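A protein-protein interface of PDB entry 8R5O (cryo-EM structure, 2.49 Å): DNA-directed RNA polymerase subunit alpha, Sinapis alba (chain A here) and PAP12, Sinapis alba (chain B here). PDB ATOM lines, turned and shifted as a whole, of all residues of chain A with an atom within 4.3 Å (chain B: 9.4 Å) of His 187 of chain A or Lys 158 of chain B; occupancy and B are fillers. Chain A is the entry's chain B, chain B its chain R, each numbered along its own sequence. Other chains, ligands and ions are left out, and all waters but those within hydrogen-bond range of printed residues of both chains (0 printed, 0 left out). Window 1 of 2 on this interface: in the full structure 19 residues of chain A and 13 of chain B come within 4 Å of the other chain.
Of chain A, only His 187, Ser 188 and Tyr 189 come within 4 Å of Lys 158 of chain B.
Printed residues of chain A within 4 Å of Tyr 150 of chain B: Tyr 189 (3.7 Å), Ile 198 (3.5 Å) and Phe 200 (3.5 Å).
Printed residues of chain A within 4 Å of Pro 152 of chain B: Tyr 189 (3.6 Å) and Gln 196 (3.4 Å).
Glu 77 of chain B touches none of the printed residues of chain A.
Of the 17 printed residues of chain B, 7 touch a printed residue of chain A.
Hydrophobic or aromatic side chains of chain B that line the printed part of chain A: Tyr 150, Pro 152 and Tyr 156.
Along chain A the printed residues that touch a printed residue of chain B span positions 187 to 200.
CE of Lys 158 of chain B touches CD2 of His 187 of chain A, at 3.8 Å.
Leu 157 of chain B touches Ser 188 of chain A.
O of Ser 188 of chain A touches CA of Lys 158 of chain B, 3.6 Å away.
Tyr 189 of chain A touches Tyr 150 of chain B.
CB of Tyr 189 of chain A touches CD1 of Tyr 156 of chain B (3.8 Å).
Tyr 189 of chain A touches Leu 157 of chain B (CA to O, 3.4 Å).
Tyr 189 of chain A touches Lys 158 of chain B.
Tyr 189 of chain A touches Glu 159 of chain B (C to OE2, 3.7 Å).
Gln 196 of chain A touches Tyr 156 of chain B (NE2 to OH, 3.7 Å).
CZ of Phe 200 of chain A touches CD2 of Tyr 150 of chain B (3.5 Å).
O of His 187 of chain A lies within hydrogen-bond range of N of Ile 198 of chain A, at 2.7 Å.
The backbone NH (N) of Tyr 189 of chain A sits at hydrogen-bond distance from the backbone carbonyl oxygen (O) of Gln 196 of chain A, 2.7 Å away.
OD1 of Asp 148 of chain B is in hydrogen-bond range of N of Tyr 150 of chain B (2.6 Å).
OD1 of Asp 148 of chain B lies within hydrogen-bond range of N of Lys 151 of chain B (3.3 Å).
The backbone carbonyl oxygen of Ser 188 of chain A sits at hydrogen-bond distance from the backbone NH of Glu 159 of chain B, at 2.8 Å.
OH of Tyr 189 of chain A lies within hydrogen-bond range of OD2 of Asp 148 of chain B.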
ATOM      1  N   ILE A 186     -13.778   5.120  30.582  1.00  0.00           N
ATOM      2  CA  ILE A 186     -13.909   3.831  29.915  1.00  0.00           C
ATOM      3  C   ILE A 186     -15.257   3.226  30.274  1.00  0.00           C
ATOM      4  O   ILE A 186     -15.621   3.168  31.453  1.00  0.00           O
ATOM      5  CB  ILE A 186     -12.771   2.871  30.304  1.00  0.00           C
ATOM      6  CG1 ILE A 186     -11.416   3.517  30.020  1.00  0.00           C
ATOM      7  CG2 ILE A 186     -12.905   1.557  29.557  1.00  0.00           C
ATOM      8  CD1 ILE A 186     -10.260   2.771  30.610  1.00  0.00           C
ATOM      9  N   HIS A 187     -15.992   2.781  29.263  1.00  0.00           N
ATOM     10  CA  HIS A 187     -17.215   2.018  29.452  1.00  0.00           C
ATOM     11  C   HIS A 187     -16.972   0.579  29.023  1.00  0.00           C
ATOM     12  O   HIS A 187     -16.367   0.331  27.978  1.00  0.00           O
ATOM     13  CB  HIS A 187     -18.376   2.608  28.649  1.00  0.00           C
ATOM     14  CG  HIS A 187     -18.812   3.963  29.115  1.00  0.00           C
ATOM     15  ND1 HIS A 187     -18.109   4.695  30.047  1.00  0.00           N
ATOM     16  CD2 HIS A 187     -19.882   4.718  28.773  1.00  0.00           C
ATOM     17  CE1 HIS A 187     -18.726   5.843  30.259  1.00  0.00           C
ATOM     18  NE2 HIS A 187     -19.805   5.881  29.498  1.00  0.00           N
ATOM     19  N   SER A 188     -17.438  -0.363  29.831  1.00  0.00           N
ATOM     20  CA  SER A 188     -17.287  -1.781  29.543  1.00  0.00           C
ATOM     21  C   SER A 188     -18.648  -2.398  29.260  1.00  0.00           C
ATOM     22  O   SER A 188     -19.612  -2.168  29.996  1.00  0.00           O
ATOM     23  CB  SER A 188     -16.612  -2.511  30.705  1.00  0.00           C
ATOM     24  OG  SER A 188     -15.324  -1.980  30.959  1.00  0.00           O
ATOM     25  N   TYR A 189     -18.718  -3.179  28.189  1.00  0.00           N
ATOM     26  CA  TYR A 189     -19.928  -3.888  27.811  1.00  0.00           C
ATOM     27  C   TYR A 189     -19.604  -5.365  27.652  1.00  0.00           C
ATOM     28  O   TYR A 189     -18.458  -5.748  27.411  1.00  0.00           O
ATOM     29  CB  TYR A 189     -20.527  -3.336  26.513  1.00  0.00           C
ATOM     30  CG  TYR A 189     -20.976  -1.899  26.617  1.00  0.00           C
ATOM     31  CD1 TYR A 189     -20.089  -0.857  26.394  1.00  0.00           C
ATOM     32  CD2 TYR A 189     -22.288  -1.585  26.939  1.00  0.00           C
ATOM     33  CE1 TYR A 189     -20.497   0.460  26.490  1.00  0.00           C
ATOM     34  CE2 TYR A 189     -22.703  -0.274  27.037  1.00  0.00           C
ATOM     35  CZ  TYR A 189     -21.805   0.744  26.812  1.00  0.00           C
ATOM     36  OH  TYR A 189     -22.221   2.050  26.909  1.00  0.00           O
ATOM     37  N   GLN A 196     -15.962  -6.158  25.820  1.00  0.00           N
ATOM     38  CA  GLN A 196     -15.698  -5.064  24.892  1.00  0.00           C
ATOM     39  C   GLN A 196     -15.735  -3.734  25.633  1.00  0.00           C
ATOM     40  O   GLN A 196     -16.701  -3.446  26.344  1.00  0.00           O
ATOM     41  CB  GLN A 196     -16.721  -5.080  23.755  1.00  0.00           C
ATOM     42  CG  GLN A 196     -16.683  -3.868  22.852  1.00  0.00           C
ATOM     43  CD  GLN A 196     -17.658  -3.984  21.697  1.00  0.00           C
ATOM     44  OE1 GLN A 196     -18.204  -2.986  21.231  1.00  0.00           O
ATOM     45  NE2 GLN A 196     -17.877  -5.206  21.228  1.00  0.00           N
ATOM     46  N   GLU A 197     -14.700  -2.912  25.479  1.00  0.00           N
ATOM     47  CA  GLU A 197     -14.628  -1.641  26.182  1.00  0.00           C
ATOM     48  C   GLU A 197     -14.569  -0.484  25.194  1.00  0.00           C
ATOM     49  O   GLU A 197     -14.088  -0.625  24.067  1.00  0.00           O
ATOM     50  CB  GLU A 197     -13.424  -1.585  27.135  1.00  0.00           C
ATOM     51  CG  GLU A 197     -12.066  -1.532  26.468  1.00  0.00           C
ATOM     52  CD  GLU A 197     -10.931  -1.597  27.473  1.00  0.00           C
ATOM     53  OE1 GLU A 197     -11.192  -1.963  28.637  1.00  0.00           O
ATOM     54  OE2 GLU A 197      -9.782  -1.279  27.105  1.00  0.00           O
ATOM     55  N   ILE A 198     -15.071   0.664  25.637  1.00  0.00           N
ATOM     56  CA  ILE A 198     -15.179   1.864  24.819  1.00  0.00           C
ATOM     57  C   ILE A 198     -14.442   2.991  25.525  1.00  0.00           C
ATOM     58  O   ILE A 198     -14.634   3.206  26.727  1.00  0.00           O
ATOM     59  CB  ILE A 198     -16.650   2.239  24.567  1.00  0.00           C
ATOM     60  CG1 ILE A 198     -17.344   1.139  23.762  1.00  0.00           C
ATOM     61  CG2 ILE A 198     -16.748   3.568  23.860  1.00  0.00           C
ATOM     62  CD1 ILE A 198     -18.777   1.448  23.428  1.00  0.00           C
ATOM     63  N   PHE A 200     -13.618   6.985  25.940  1.00  0.00           N
ATOM     64  CA  PHE A 200     -14.026   8.365  25.730  1.00  0.00           C
ATOM     65  C   PHE A 200     -12.881   9.292  26.110  1.00  0.00           C
ATOM     66  O   PHE A 200     -12.191   9.060  27.105  1.00  0.00           O
ATOM     67  CB  PHE A 200     -15.269   8.715  26.554  1.00  0.00           C
ATOM     68  CG  PHE A 200     -16.516   8.013  26.105  1.00  0.00           C
ATOM     69  CD1 PHE A 200     -17.312   8.555  25.113  1.00  0.00           C
ATOM     70  CD2 PHE A 200     -16.897   6.813  26.681  1.00  0.00           C
ATOM     71  CE1 PHE A 200     -18.462   7.912  24.700  1.00  0.00           C
ATOM     72  CE2 PHE A 200     -18.046   6.166  26.271  1.00  0.00           C
ATOM     73  CZ  PHE A 200     -18.828   6.716  25.281  1.00  0.00           C
ATOM     74  N   GLU B  70     -18.105  16.950  32.327  1.00  0.00           N
ATOM     75  CA  GLU B  70     -18.088  15.583  32.837  1.00  0.00           C
ATOM     76  C   GLU B  70     -18.942  15.460  34.091  1.00  0.00           C
ATOM     77  O   GLU B  70     -19.658  14.469  34.273  1.00  0.00           O
ATOM     78  CB  GLU B  70     -16.651  15.148  33.121  1.00  0.00           C
ATOM     79  CG  GLU B  70     -16.386  13.674  32.863  1.00  0.00           C
ATOM     80  CD  GLU B  70     -17.124  12.763  33.821  1.00  0.00           C
ATOM     81  OE1 GLU B  70     -17.069  13.014  35.044  1.00  0.00           O
ATOM     82  OE2 GLU B  70     -17.763  11.801  33.349  1.00  0.00           O
ATOM     83  N   ARG B  73     -22.794  15.719  33.150  1.00  0.00           N
ATOM     84  CA  ARG B  73     -23.287  14.492  32.538  1.00  0.00           C
ATOM     85  C   ARG B  73     -23.380  13.356  33.550  1.00  0.00           C
ATOM     86  O   ARG B  73     -24.275  12.511  33.444  1.00  0.00           O
ATOM     87  CB  ARG B  73     -22.400  14.111  31.350  1.00  0.00           C
ATOM     88  CG  ARG B  73     -21.867  12.689  31.363  1.00  0.00           C
ATOM     89  CD  ARG B  73     -21.300  12.302  30.006  1.00  0.00           C
ATOM     90  NE  ARG B  73     -20.544  13.387  29.393  1.00  0.00           N
ATOM     91  CZ  ARG B  73     -19.253  13.611  29.594  1.00  0.00           C
ATOM     92  NH1 ARG B  73     -18.536  12.849  30.402  1.00  0.00           N
ATOM     93  NH2 ARG B  73     -18.666  14.626  28.967  1.00  0.00           N
ATOM     94  N   LYS B  74     -22.491  13.329  34.545  1.00  0.00           N
ATOM     95  CA  LYS B  74     -22.576  12.297  35.573  1.00  0.00           C
ATOM     96  C   LYS B  74     -23.742  12.549  36.521  1.00  0.00           C
ATOM     97  O   LYS B  74     -24.351  11.600  37.027  1.00  0.00           O
ATOM     98  CB  LYS B  74     -21.265  12.208  36.352  1.00  0.00           C
ATOM     99  CG  LYS B  74     -20.177  11.423  35.644  1.00  0.00           C
ATOM    100  CD  LYS B  74     -19.079  11.013  36.609  1.00  0.00           C
ATOM    101  CE  LYS B  74     -18.120  10.025  35.965  1.00  0.00           C
ATOM    102  NZ  LYS B  74     -17.117   9.509  36.934  1.00  0.00           N
ATOM    103  N   GLU B  77     -26.656  11.100  34.910  1.00  0.00           N
ATOM    104  CA  GLU B  77     -26.571   9.643  34.843  1.00  0.00           C
ATOM    105  C   GLU B  77     -26.980   8.995  36.159  1.00  0.00           C
ATOM    106  O   GLU B  77     -27.652   7.957  36.165  1.00  0.00           O
ATOM    107  CB  GLU B  77     -25.156   9.212  34.457  1.00  0.00           C
ATOM    108  CG  GLU B  77     -24.810   9.439  32.994  1.00  0.00           C
ATOM    109  CD  GLU B  77     -23.359   9.119  32.681  1.00  0.00           C
ATOM    110  OE1 GLU B  77     -22.668   8.563  33.559  1.00  0.00           O
ATOM    111  OE2 GLU B  77     -22.912   9.426  31.557  1.00  0.00           O
ATOM    112  N   SER B 147     -31.329   6.676  28.300  1.00  0.00           N
ATOM    113  CA  SER B 147     -30.715   5.446  27.822  1.00  0.00           C
ATOM    114  C   SER B 147     -29.321   5.738  27.286  1.00  0.00           C
ATOM    115  O   SER B 147     -29.007   6.862  26.887  1.00  0.00           O
ATOM    116  CB  SER B 147     -31.569   4.775  26.737  1.00  0.00           C
ATOM    117  OG  SER B 147     -31.785   5.652  25.645  1.00  0.00           O
ATOM    118  N   ASP B 148     -28.486   4.704  27.285  1.00  0.00           N
ATOM    119  CA  ASP B 148     -27.121   4.830  26.789  1.00  0.00           C
ATOM    120  C   ASP B 148     -27.122   4.790  25.266  1.00  0.00           C
ATOM    121  O   ASP B 148     -27.575   3.797  24.684  1.00  0.00           O
ATOM    122  CB  ASP B 148     -26.249   3.712  27.352  1.00  0.00           C
ATOM    123  CG  ASP B 148     -24.771   3.915  27.065  1.00  0.00           C
ATOM    124  OD1 ASP B 148     -24.382   3.932  25.879  1.00  0.00           O
ATOM    125  OD2 ASP B 148     -23.996   4.065  28.032  1.00  0.00           O
ATOM    126  N   PRO B 149     -26.634   5.832  24.586  1.00  0.00           N
ATOM    127  CA  PRO B 149     -26.596   5.806  23.119  1.00  0.00           C
ATOM    128  C   PRO B 149     -25.411   5.051  22.539  1.00  0.00           C
ATOM    129  O   PRO B 149     -25.390   4.814  21.323  1.00  0.00           O
ATOM    130  CB  PRO B 149     -26.527   7.291  22.752  1.00  0.00           C
ATOM    131  CG  PRO B 149     -25.803   7.909  23.902  1.00  0.00           C
ATOM    132  CD  PRO B 149     -26.217   7.137  25.130  1.00  0.00           C
ATOM    133  N   TYR B 150     -24.432   4.663  23.356  1.00  0.00           N
ATOM    134  CA  TYR B 150     -23.229   3.995  22.878  1.00  0.00           C
ATOM    135  C   TYR B 150     -23.260   2.492  23.126  1.00  0.00           C
ATOM    136  O   TYR B 150     -22.202   1.857  23.181  1.00  0.00           O
ATOM    137  CB  TYR B 150     -21.993   4.616  23.530  1.00  0.00           C
ATOM    138  CG  TYR B 150     -22.067   6.120  23.653  1.00  0.00           C
ATOM    139  CD1 TYR B 150     -21.875   6.939  22.549  1.00  0.00           C
ATOM    140  CD2 TYR B 150     -22.335   6.723  24.874  1.00  0.00           C
ATOM    141  CE1 TYR B 150     -21.946   8.314  22.659  1.00  0.00           C
ATOM    142  CE2 TYR B 150     -22.404   8.094  24.995  1.00  0.00           C
ATOM    143  CZ  TYR B 150     -22.211   8.886  23.883  1.00  0.00           C
ATOM    144  OH  TYR B 150     -22.282  10.254  24.002  1.00  0.00           O
ATOM    145  N   LYS B 151     -24.445   1.915  23.280  1.00  0.00           N
ATOM    146  CA  LYS B 151     -24.554   0.479  23.495  1.00  0.00           C
ATOM    147  C   LYS B 151     -24.262  -0.256  22.192  1.00  0.00           C
ATOM    148  O   LYS B 151     -24.890   0.034  21.167  1.00  0.00           O
ATOM    149  CB  LYS B 151     -25.948   0.125  24.006  1.00  0.00           C
ATOM    150  CG  LYS B 151     -26.096  -1.311  24.474  1.00  0.00           C
ATOM    151  CD  LYS B 151     -27.549  -1.674  24.757  1.00  0.00           C
ATOM    152  CE  LYS B 151     -28.153  -0.815  25.860  1.00  0.00           C
ATOM    153  NZ  LYS B 151     -28.835   0.405  25.342  1.00  0.00           N
ATOM    154  N   PRO B 152     -23.326  -1.208  22.183  1.00  0.00           N
ATOM    155  CA  PRO B 152     -22.910  -1.880  20.944  1.00  0.00           C
ATOM    156  C   PRO B 152     -23.878  -2.961  20.460  1.00  0.00           C
ATOM    157  O   PRO B 152     -23.474  -4.071  20.112  1.00  0.00           O
ATOM    158  CB  PRO B 152     -21.550  -2.471  21.326  1.00  0.00           C
ATOM    159  CG  PRO B 152     -21.673  -2.750  22.774  1.00  0.00           C
ATOM    160  CD  PRO B 152     -22.540  -1.658  23.344  1.00  0.00           C
ATOM    161  N   GLY B 153     -25.165  -2.628  20.425  1.00  0.00           N
ATOM    162  CA  GLY B 153     -26.168  -3.527  19.907  1.00  0.00           C
ATOM    163  C   GLY B 153     -26.866  -4.336  20.981  1.00  0.00           C
ATOM    164  O   GLY B 153     -26.566  -4.225  22.174  1.00  0.00           O
ATOM    165  N   GLY B 155     -28.124  -7.404  23.412  1.00  0.00           N
ATOM    166  CA  GLY B 155     -27.431  -8.398  24.193  1.00  0.00           C
ATOM    167  C   GLY B 155     -26.338  -7.858  25.090  1.00  0.00           C
ATOM    168  O   GLY B 155     -25.903  -8.561  26.008  1.00  0.00           O
ATOM    169  N   TYR B 156     -25.891  -6.625  24.863  1.00  0.00           N
ATOM    170  CA  TYR B 156     -24.780  -6.050  25.609  1.00  0.00           C
ATOM    171  C   TYR B 156     -25.310  -5.257  26.796  1.00  0.00           C
ATOM    172  O   TYR B 156     -26.153  -4.370  26.632  1.00  0.00           O
ATOM    173  CB  TYR B 156     -23.931  -5.155  24.708  1.00  0.00           C
ATOM    174  CG  TYR B 156     -22.965  -5.912  23.830  1.00  0.00           C
ATOM    175  CD1 TYR B 156     -21.686  -6.211  24.274  1.00  0.00           C
ATOM    176  CD2 TYR B 156     -23.331  -6.327  22.557  1.00  0.00           C
ATOM    177  CE1 TYR B 156     -20.798  -6.899  23.477  1.00  0.00           C
ATOM    178  CE2 TYR B 156     -22.447  -7.018  21.751  1.00  0.00           C
ATOM    179  CZ  TYR B 156     -21.181  -7.301  22.218  1.00  0.00           C
ATOM    180  OH  TYR B 156     -20.294  -7.989  21.426  1.00  0.00           O
ATOM    181  N   LEU B 157     -24.814  -5.579  27.984  1.00  0.00           N
ATOM    182  CA  LEU B 157     -25.124  -4.833  29.196  1.00  0.00           C
ATOM    183  C   LEU B 157     -23.925  -3.980  29.579  1.00  0.00           C
ATOM    184  O   LEU B 157     -22.792  -4.470  29.593  1.00  0.00           O
ATOM    185  CB  LEU B 157     -25.474  -5.768  30.352  1.00  0.00           C
ATOM    186  CG  LEU B 157     -26.709  -6.658  30.250  1.00  0.00           C
ATOM    187  CD1 LEU B 157     -26.951  -7.313  31.590  1.00  0.00           C
ATOM    188  CD2 LEU B 157     -27.918  -5.856  29.821  1.00  0.00           C
ATOM    189  N   LYS B 158     -24.175  -2.711  29.885  1.00  0.00           N
ATOM    190  CA  LYS B 158     -23.127  -1.884  30.462  1.00  0.00           C
ATOM    191  C   LYS B 158     -22.732  -2.445  31.821  1.00  0.00           C
ATOM    192  O   LYS B 158     -23.590  -2.767  32.647  1.00  0.00           O
ATOM    193  CB  LYS B 158     -23.598  -0.437  30.593  1.00  0.00           C
ATOM    194  CG  LYS B 158     -22.491   0.532  30.960  1.00  0.00           C
ATOM    195  CD  LYS B 158     -23.003   1.957  31.036  1.00  0.00           C
ATOM    196  CE  LYS B 158     -21.887   2.915  31.407  1.00  0.00           C
ATOM    197  NZ  LYS B 158     -21.232   2.530  32.687  1.00  0.00           N
ATOM    198  N   GLU B 159     -21.430  -2.562  32.052  1.00  0.00           N
ATOM    199  CA  GLU B 159     -20.896  -3.199  33.246  1.00  0.00           C
ATOM    200  C   GLU B 159     -20.325  -2.139  34.175  1.00  0.00           C
ATOM    201  O   GLU B 159     -19.538  -1.290  33.745  1.00  0.00           O
ATOM    202  CB  GLU B 159     -19.826  -4.227  32.881  1.00  0.00           C
ATOM    203  CG  GLU B 159     -20.325  -5.319  31.952  1.00  0.00           C
ATOM    204  CD  GLU B 159     -19.213  -6.212  31.444  1.00  0.00           C
ATOM    205  OE1 GLU B 159     -18.031  -5.861  31.641  1.00  0.00           O
ATOM    206  OE2 GLU B 159     -19.520  -7.266  30.852  1.00  0.00           O
ATOM    207  N   TYR B 160     -20.721  -2.194  35.441  1.00  0.00           N
ATOM    208  CA  TYR B 160     -20.288  -1.208  36.419  1.00  0.00           C
ATOM    209  C   TYR B 160     -19.028  -1.667  37.144  1.00  0.00           C
ATOM    210  O   TYR B 160     -18.996  -2.750  37.725  1.00  0.00           O
ATOM    211  CB  TYR B 160     -21.405  -0.932  37.425  1.00  0.00           C
ATOM    212  CG  TYR B 160     -21.187   0.315  38.245  1.00  0.00           C
ATOM    213  CD1 TYR B 160     -21.591   1.556  37.772  1.00  0.00           C
ATOM    214  CD2 TYR B 160     -20.577   0.256  39.490  1.00  0.00           C
ATOM    215  CE1 TYR B 160     -21.395   2.700  38.515  1.00  0.00           C
ATOM    216  CE2 TYR B 160     -20.378   1.397  40.241  1.00  0.00           C
ATOM    217  CZ  TYR B 160     -20.788   2.615  39.747  1.00  0.00           C
ATOM    218  OH  TYR B 160     -20.594   3.758  40.485  1.00  0.00           O
